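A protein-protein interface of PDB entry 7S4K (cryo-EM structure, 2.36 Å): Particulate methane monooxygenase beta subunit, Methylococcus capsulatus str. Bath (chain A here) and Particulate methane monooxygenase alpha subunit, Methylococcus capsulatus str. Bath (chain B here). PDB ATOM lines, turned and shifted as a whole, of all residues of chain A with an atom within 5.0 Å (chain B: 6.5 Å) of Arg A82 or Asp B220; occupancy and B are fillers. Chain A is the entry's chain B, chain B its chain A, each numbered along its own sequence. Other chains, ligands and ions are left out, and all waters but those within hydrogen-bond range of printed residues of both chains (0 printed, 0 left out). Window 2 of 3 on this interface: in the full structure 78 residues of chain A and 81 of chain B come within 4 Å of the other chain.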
ATOM      1  N   TYR A  78      11.378 -27.398  15.717  1.00  0.00           N
ATOM      2  CA  TYR A  78      12.423 -26.453  15.334  1.00  0.00           C
ATOM      3  C   TYR A  78      12.350 -26.102  13.851  1.00  0.00           C
ATOM      4  O   TYR A  78      12.284 -24.924  13.481  1.00  0.00           O
ATOM      5  CB  TYR A  78      13.797 -27.018  15.685  1.00  0.00           C
ATOM      6  CG  TYR A  78      14.947 -26.259  15.068  1.00  0.00           C
ATOM      7  CD1 TYR A  78      15.268 -24.982  15.499  1.00  0.00           C
ATOM      8  CD2 TYR A  78      15.721 -26.825  14.068  1.00  0.00           C
ATOM      9  CE1 TYR A  78      16.318 -24.287  14.944  1.00  0.00           C
ATOM     10  CE2 TYR A  78      16.774 -26.137  13.509  1.00  0.00           C
ATOM     11  CZ  TYR A  78      17.067 -24.869  13.951  1.00  0.00           C
ATOM     12  OH  TYR A  78      18.116 -24.176  13.397  1.00  0.00           O
ATOM     13  N   LEU A  79      12.364 -27.119  12.987  1.00  0.00           N
ATOM     14  CA  LEU A  79      12.512 -26.891  11.555  1.00  0.00           C
ATOM     15  C   LEU A  79      11.309 -26.163  10.976  1.00  0.00           C
ATOM     16  O   LEU A  79      11.464 -25.172  10.258  1.00  0.00           O
ATOM     17  CB  LEU A  79      12.731 -28.220  10.835  1.00  0.00           C
ATOM     18  CG  LEU A  79      14.140 -28.799  10.921  1.00  0.00           C
ATOM     19  CD1 LEU A  79      14.229 -30.080  10.122  1.00  0.00           C
ATOM     20  CD2 LEU A  79      15.160 -27.792  10.431  1.00  0.00           C
ATOM     21  N   TRP A  80      10.096 -26.638  11.268  1.00  0.00           N
ATOM     22  CA  TRP A  80       8.918 -25.976  10.723  1.00  0.00           C
ATOM     23  C   TRP A  80       8.822 -24.541  11.218  1.00  0.00           C
ATOM     24  O   TRP A  80       8.618 -23.615  10.429  1.00  0.00           O
ATOM     25  CB  TRP A  80       7.658 -26.755  11.087  1.00  0.00           C
ATOM     26  CG  TRP A  80       6.412 -26.108  10.582  1.00  0.00           C
ATOM     27  CD1 TRP A  80       5.443 -25.507  11.327  1.00  0.00           C
ATOM     28  CD2 TRP A  80       6.000 -25.988   9.218  1.00  0.00           C
ATOM     29  NE1 TRP A  80       4.453 -25.022  10.512  1.00  0.00           N
ATOM     30  CE2 TRP A  80       4.773 -25.305   9.212  1.00  0.00           C
ATOM     31  CE3 TRP A  80       6.553 -26.394   8.001  1.00  0.00           C
ATOM     32  CZ2 TRP A  80       4.086 -25.019   8.038  1.00  0.00           C
ATOM     33  CZ3 TRP A  80       5.871 -26.108   6.839  1.00  0.00           C
ATOM     34  CH2 TRP A  80       4.652 -25.427   6.865  1.00  0.00           C
ATOM     35  N   GLU A  81       9.025 -24.335  12.519  1.00  0.00           N
ATOM     36  CA  GLU A  81       8.892 -22.998  13.085  1.00  0.00           C
ATOM     37  C   GLU A  81       9.913 -22.027  12.512  1.00  0.00           C
ATOM     38  O   GLU A  81       9.573 -20.874  12.228  1.00  0.00           O
ATOM     39  CB  GLU A  81       9.024 -23.053  14.606  1.00  0.00           C
ATOM     40  CG  GLU A  81       8.528 -21.814  15.355  1.00  0.00           C
ATOM     41  CD  GLU A  81       7.017 -21.598  15.294  1.00  0.00           C
ATOM     42  OE1 GLU A  81       6.360 -22.013  14.318  1.00  0.00           O
ATOM     43  OE2 GLU A  81       6.479 -20.998  16.247  1.00  0.00           O
ATOM     44  N   ARG A  82      11.162 -22.457  12.329  1.00  0.00           N
ATOM     45  CA  ARG A  82      12.207 -21.514  11.959  1.00  0.00           C
ATOM     46  C   ARG A  82      12.455 -21.411  10.461  1.00  0.00           C
ATOM     47  O   ARG A  82      13.004 -20.399  10.019  1.00  0.00           O
ATOM     48  CB  ARG A  82      13.521 -21.876  12.658  1.00  0.00           C
ATOM     49  CG  ARG A  82      13.485 -21.711  14.165  1.00  0.00           C
ATOM     50  CD  ARG A  82      12.832 -20.399  14.566  1.00  0.00           C
ATOM     51  NE  ARG A  82      13.583 -19.243  14.090  1.00  0.00           N
ATOM     52  CZ  ARG A  82      14.588 -18.680  14.745  1.00  0.00           C
ATOM     53  NH1 ARG A  82      14.994 -19.141  15.915  1.00  0.00           N
ATOM     54  NH2 ARG A  82      15.200 -17.627  14.213  1.00  0.00           N
ATOM     55  N   TYR A  83      12.072 -22.411   9.665  1.00  0.00           N
ATOM     56  CA  TYR A  83      12.352 -22.372   8.239  1.00  0.00           C
ATOM     57  C   TYR A  83      11.182 -22.808   7.371  1.00  0.00           C
ATOM     58  O   TYR A  83      11.315 -22.776   6.144  1.00  0.00           O
ATOM     59  CB  TYR A  83      13.564 -23.258   7.901  1.00  0.00           C
ATOM     60  CG  TYR A  83      14.730 -23.155   8.857  1.00  0.00           C
ATOM     61  CD1 TYR A  83      14.773 -23.914  10.017  1.00  0.00           C
ATOM     62  CD2 TYR A  83      15.803 -22.323   8.583  1.00  0.00           C
ATOM     63  CE1 TYR A  83      15.840 -23.827  10.886  1.00  0.00           C
ATOM     64  CE2 TYR A  83      16.873 -22.234   9.444  1.00  0.00           C
ATOM     65  CZ  TYR A  83      16.886 -22.985  10.593  1.00  0.00           C
ATOM     66  OH  TYR A  83      17.954 -22.896  11.453  1.00  0.00           O
ATOM     67  N   ARG A  84      10.052 -23.209   7.954  1.00  0.00           N
ATOM     68  CA  ARG A  84       8.950 -23.816   7.210  1.00  0.00           C
ATOM     69  C   ARG A  84       9.435 -25.014   6.400  1.00  0.00           C
ATOM     70  O   ARG A  84       9.086 -25.185   5.231  1.00  0.00           O
ATOM     71  CB  ARG A  84       8.251 -22.790   6.320  1.00  0.00           C
ATOM     72  CG  ARG A  84       7.535 -21.701   7.090  1.00  0.00           C
ATOM     73  CD  ARG A  84       6.200 -22.197   7.609  1.00  0.00           C
ATOM     74  NE  ARG A  84       5.582 -21.263   8.542  1.00  0.00           N
ATOM     75  CZ  ARG A  84       5.991 -21.058   9.785  1.00  0.00           C
ATOM     76  NH1 ARG A  84       7.019 -21.717  10.293  1.00  0.00           N
ATOM     77  NH2 ARG A  84       5.350 -20.173  10.540  1.00  0.00           N
ATOM     78  N   GLU A 241      18.636 -19.644  21.707  1.00  0.00           N
ATOM     79  CA  GLU A 241      19.844 -18.998  21.204  1.00  0.00           C
ATOM     80  C   GLU A 241      20.436 -18.069  22.250  1.00  0.00           C
ATOM     81  O   GLU A 241      21.020 -17.032  21.926  1.00  0.00           O
ATOM     82  CB  GLU A 241      19.555 -18.228  19.920  1.00  0.00           C
ATOM     83  CG  GLU A 241      18.848 -19.034  18.859  1.00  0.00           C
ATOM     84  CD  GLU A 241      17.784 -18.232  18.141  1.00  0.00           C
ATOM     85  OE1 GLU A 241      18.145 -17.313  17.379  1.00  0.00           O
ATOM     86  OE2 GLU A 241      16.586 -18.521  18.339  1.00  0.00           O
ATOM     87  N   PHE B 212      18.283 -23.357   4.182  1.00  0.00           N
ATOM     88  CA  PHE B 212      18.444 -22.916   5.565  1.00  0.00           C
ATOM     89  C   PHE B 212      18.429 -21.401   5.746  1.00  0.00           C
ATOM     90  O   PHE B 212      17.533 -20.873   6.407  1.00  0.00           O
ATOM     91  CB  PHE B 212      19.735 -23.505   6.145  1.00  0.00           C
ATOM     92  CG  PHE B 212      19.618 -24.949   6.524  1.00  0.00           C
ATOM     93  CD1 PHE B 212      18.779 -25.339   7.551  1.00  0.00           C
ATOM     94  CD2 PHE B 212      20.344 -25.916   5.856  1.00  0.00           C
ATOM     95  CE1 PHE B 212      18.664 -26.665   7.903  1.00  0.00           C
ATOM     96  CE2 PHE B 212      20.235 -27.243   6.205  1.00  0.00           C
ATOM     97  CZ  PHE B 212      19.394 -27.618   7.229  1.00  0.00           C
ATOM     98  N   ARG B 215      15.517 -19.206   3.953  1.00  0.00           N
ATOM     99  CA  ARG B 215      14.233 -19.513   4.575  1.00  0.00           C
ATOM    100  C   ARG B 215      14.174 -18.998   6.006  1.00  0.00           C
ATOM    101  O   ARG B 215      13.133 -18.500   6.450  1.00  0.00           O
ATOM    102  CB  ARG B 215      13.971 -21.016   4.526  1.00  0.00           C
ATOM    103  CG  ARG B 215      13.546 -21.507   3.156  1.00  0.00           C
ATOM    104  CD  ARG B 215      13.262 -22.993   3.153  1.00  0.00           C
ATOM    105  NE  ARG B 215      11.914 -23.299   3.608  1.00  0.00           N
ATOM    106  CZ  ARG B 215      10.871 -23.445   2.804  1.00  0.00           C
ATOM    107  NH1 ARG B 215      10.981 -23.291   1.496  1.00  0.00           N
ATOM    108  NH2 ARG B 215       9.688 -23.752   3.326  1.00  0.00           N
ATOM    109  N   LEU B 216      15.282 -19.105   6.745  1.00  0.00           N
ATOM    110  CA  LEU B 216      15.332 -18.542   8.088  1.00  0.00           C
ATOM    111  C   LEU B 216      15.105 -17.040   8.054  1.00  0.00           C
ATOM    112  O   LEU B 216      14.339 -16.500   8.859  1.00  0.00           O
ATOM    113  CB  LEU B 216      16.678 -18.857   8.738  1.00  0.00           C
ATOM    114  CG  LEU B 216      16.968 -18.200  10.087  1.00  0.00           C
ATOM    115  CD1 LEU B 216      16.088 -18.796  11.167  1.00  0.00           C
ATOM    116  CD2 LEU B 216      18.432 -18.344  10.448  1.00  0.00           C
ATOM    117  N   LEU B 217      15.753 -16.353   7.114  1.00  0.00           N
ATOM    118  CA  LEU B 217      15.587 -14.909   7.008  1.00  0.00           C
ATOM    119  C   LEU B 217      14.171 -14.543   6.583  1.00  0.00           C
ATOM    120  O   LEU B 217      13.623 -13.539   7.046  1.00  0.00           O
ATOM    121  CB  LEU B 217      16.614 -14.338   6.034  1.00  0.00           C
ATOM    122  CG  LEU B 217      18.071 -14.445   6.482  1.00  0.00           C
ATOM    123  CD1 LEU B 217      19.009 -14.064   5.351  1.00  0.00           C
ATOM    124  CD2 LEU B 217      18.327 -13.592   7.708  1.00  0.00           C
ATOM    125  N   MET B 218      13.565 -15.334   5.696  1.00  0.00           N
ATOM    126  CA  MET B 218      12.198 -15.051   5.275  1.00  0.00           C
ATOM    127  C   MET B 218      11.211 -15.250   6.418  1.00  0.00           C
ATOM    128  O   MET B 218      10.256 -14.479   6.560  1.00  0.00           O
ATOM    129  CB  MET B 218      11.821 -15.926   4.082  1.00  0.00           C
ATOM    130  CG  MET B 218      12.456 -15.490   2.775  1.00  0.00           C
ATOM    131  SD  MET B 218      11.549 -14.168   1.953  1.00  0.00           S
ATOM    132  CE  MET B 218       9.942 -14.929   1.753  1.00  0.00           C
ATOM    133  N   VAL B 219      11.414 -16.283   7.237  1.00  0.00           N
ATOM    134  CA  VAL B 219      10.534 -16.493   8.381  1.00  0.00           C
ATOM    135  C   VAL B 219      10.738 -15.396   9.418  1.00  0.00           C
ATOM    136  O   VAL B 219       9.777 -14.908  10.023  1.00  0.00           O
ATOM    137  CB  VAL B 219      10.753 -17.893   8.982  1.00  0.00           C
ATOM    138  CG1 VAL B 219       9.966 -18.048  10.268  1.00  0.00           C
ATOM    139  CG2 VAL B 219      10.353 -18.964   7.989  1.00  0.00           C
ATOM    140  N   ASP B 220      11.988 -14.983   9.634  1.00  0.00           N
ATOM    141  CA  ASP B 220      12.283 -13.948  10.623  1.00  0.00           C
ATOM    142  C   ASP B 220      11.718 -12.598  10.191  1.00  0.00           C
ATOM    143  O   ASP B 220      10.878 -12.012  10.878  1.00  0.00           O
ATOM    144  CB  ASP B 220      13.796 -13.853  10.841  1.00  0.00           C
ATOM    145  CG  ASP B 220      14.336 -14.987  11.679  1.00  0.00           C
ATOM    146  OD1 ASP B 220      13.531 -15.815  12.152  1.00  0.00           O
ATOM    147  OD2 ASP B 220      15.569 -15.055  11.859  1.00  0.00           O
ATOM    148  N   ALA B 221      12.173 -12.098   9.045  1.00  0.00           N
ATOM    149  CA  ALA B 221      11.764 -10.794   8.549  1.00  0.00           C
ATOM    150  C   ALA B 221      10.326 -10.838   8.063  1.00  0.00           C
ATOM    151  O   ALA B 221      10.062 -11.181   6.907  1.00  0.00           O
ATOM    152  CB  ALA B 221      12.692 -10.333   7.424  1.00  0.00           C
ATOM    153  N   GLY B 222       9.393 -10.494   8.942  1.00  0.00           N
ATOM    154  CA  GLY B 222       7.992 -10.506   8.595  1.00  0.00           C
ATOM    155  C   GLY B 222       7.449 -11.915   8.503  1.00  0.00           C
ATOM    156  O   GLY B 222       8.134 -12.908   8.748  1.00  0.00           O
ATOM    157  N   ARG B 223       6.174 -11.993   8.142  1.00  0.00           N
ATOM    158  CA  ARG B 223       5.548 -13.279   7.906  1.00  0.00           C
ATOM    159  C   ARG B 223       6.244 -13.988   6.751  1.00  0.00           C
ATOM    160  O   ARG B 223       6.674 -13.368   5.775  1.00  0.00           O
ATOM    161  CB  ARG B 223       4.061 -13.102   7.599  1.00  0.00           C
ATOM    162  CG  ARG B 223       3.197 -12.877   8.827  1.00  0.00           C
ATOM    163  CD  ARG B 223       1.780 -12.494   8.436  1.00  0.00           C
ATOM    164  NE  ARG B 223       0.910 -12.351   9.597  1.00  0.00           N
ATOM    165  CZ  ARG B 223      -0.005 -11.401   9.734  1.00  0.00           C
ATOM    166  NH1 ARG B 223      -0.192 -10.483   8.800  1.00  0.00           N
ATOM    167  NH2 ARG B 223      -0.748 -11.371  10.836  1.00  0.00           N
ATOM    168  N   ALA B 224       6.374 -15.307   6.876  1.00  0.00           N
ATOM    169  CA  ALA B 224       7.018 -16.040   5.799  1.00  0.00           C
ATOM    170  C   ALA B 224       6.022 -16.297   4.683  1.00  0.00           C
ATOM    171  O   ALA B 224       6.114 -15.677   3.623  1.00  0.00           O
ATOM    172  CB  ALA B 224       7.583 -17.360   6.319  1.00  0.00           C
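The backbone carbonyl oxygen of Tyr A83 lies within hydrogen-bond range of the guanidinium group of Arg B215 (2.7 Å).
The side-chain carboxylate (OD1) of Asp B220 lies within salt-bridge range of the guanidinium group (NH2) of Arg A82 (3.2 Å).
NH2 of Arg B215 lies within hydrogen-bond range of O of Arg A84 (2.5 Å).
O of Glu A81 is in hydrogen-bond range of NH1 of Arg A84 (3.3 Å).
NH1 of Arg A84 lies within hydrogen-bond range of O of Trp A80, 2.5 Å away.
O of Leu A79 sits at hydrogen-bond distance from N of Arg A84 (3.3 Å).
The guanidinium group of Arg A82 lies within salt-bridge range of the side-chain carboxylate of Glu A241 (3.0 Å).
Among the printed residues, merely in contact across the chains: Glu A81 with Val B219 (3.5 Å), Arg A82 with Leu B216 (3.4 Å), Arg A82 with Val B219 (3.5 Å), Tyr A83 with Phe B212 (3.1 Å), Tyr A83 with Leu B216 (3.5 Å) and Tyr A83 with Val B219 (3.96 Å).
Asp B220 touches one residue of chain A.
Printed residues of chain B within 4 Å of Tyr A83: Phe B212, Arg B215, Leu B216 and Val B219.
Printed residues of chain A within 4 Å of Val B219: Glu A81, Arg A82 and Tyr A83.
The nearest printed residue of chain A that does not touch Asp B220 is Glu A81 (6.4 Å).
The nearest printed residue of chain A that does not touch Arg B215 is Arg A82 (4.04 Å).
Of the 11 printed residues of chain B, 5 touch a printed residue of chain A.
Hydrophobic or aromatic side chains of chain B within 4 Å of the printed part of chain A: Leu B216 and Val B219.
Of the 8 printed residues of chain A, 4 touch a printed residue of chain B.
Printed residues of chain A that touch a printed residue of chain B: Glu A81, Arg A82, Tyr A83 and Arg A84.
Hydrophobic or aromatic side chains of chain A within 4 Å of the printed part of chain B: Tyr A83.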
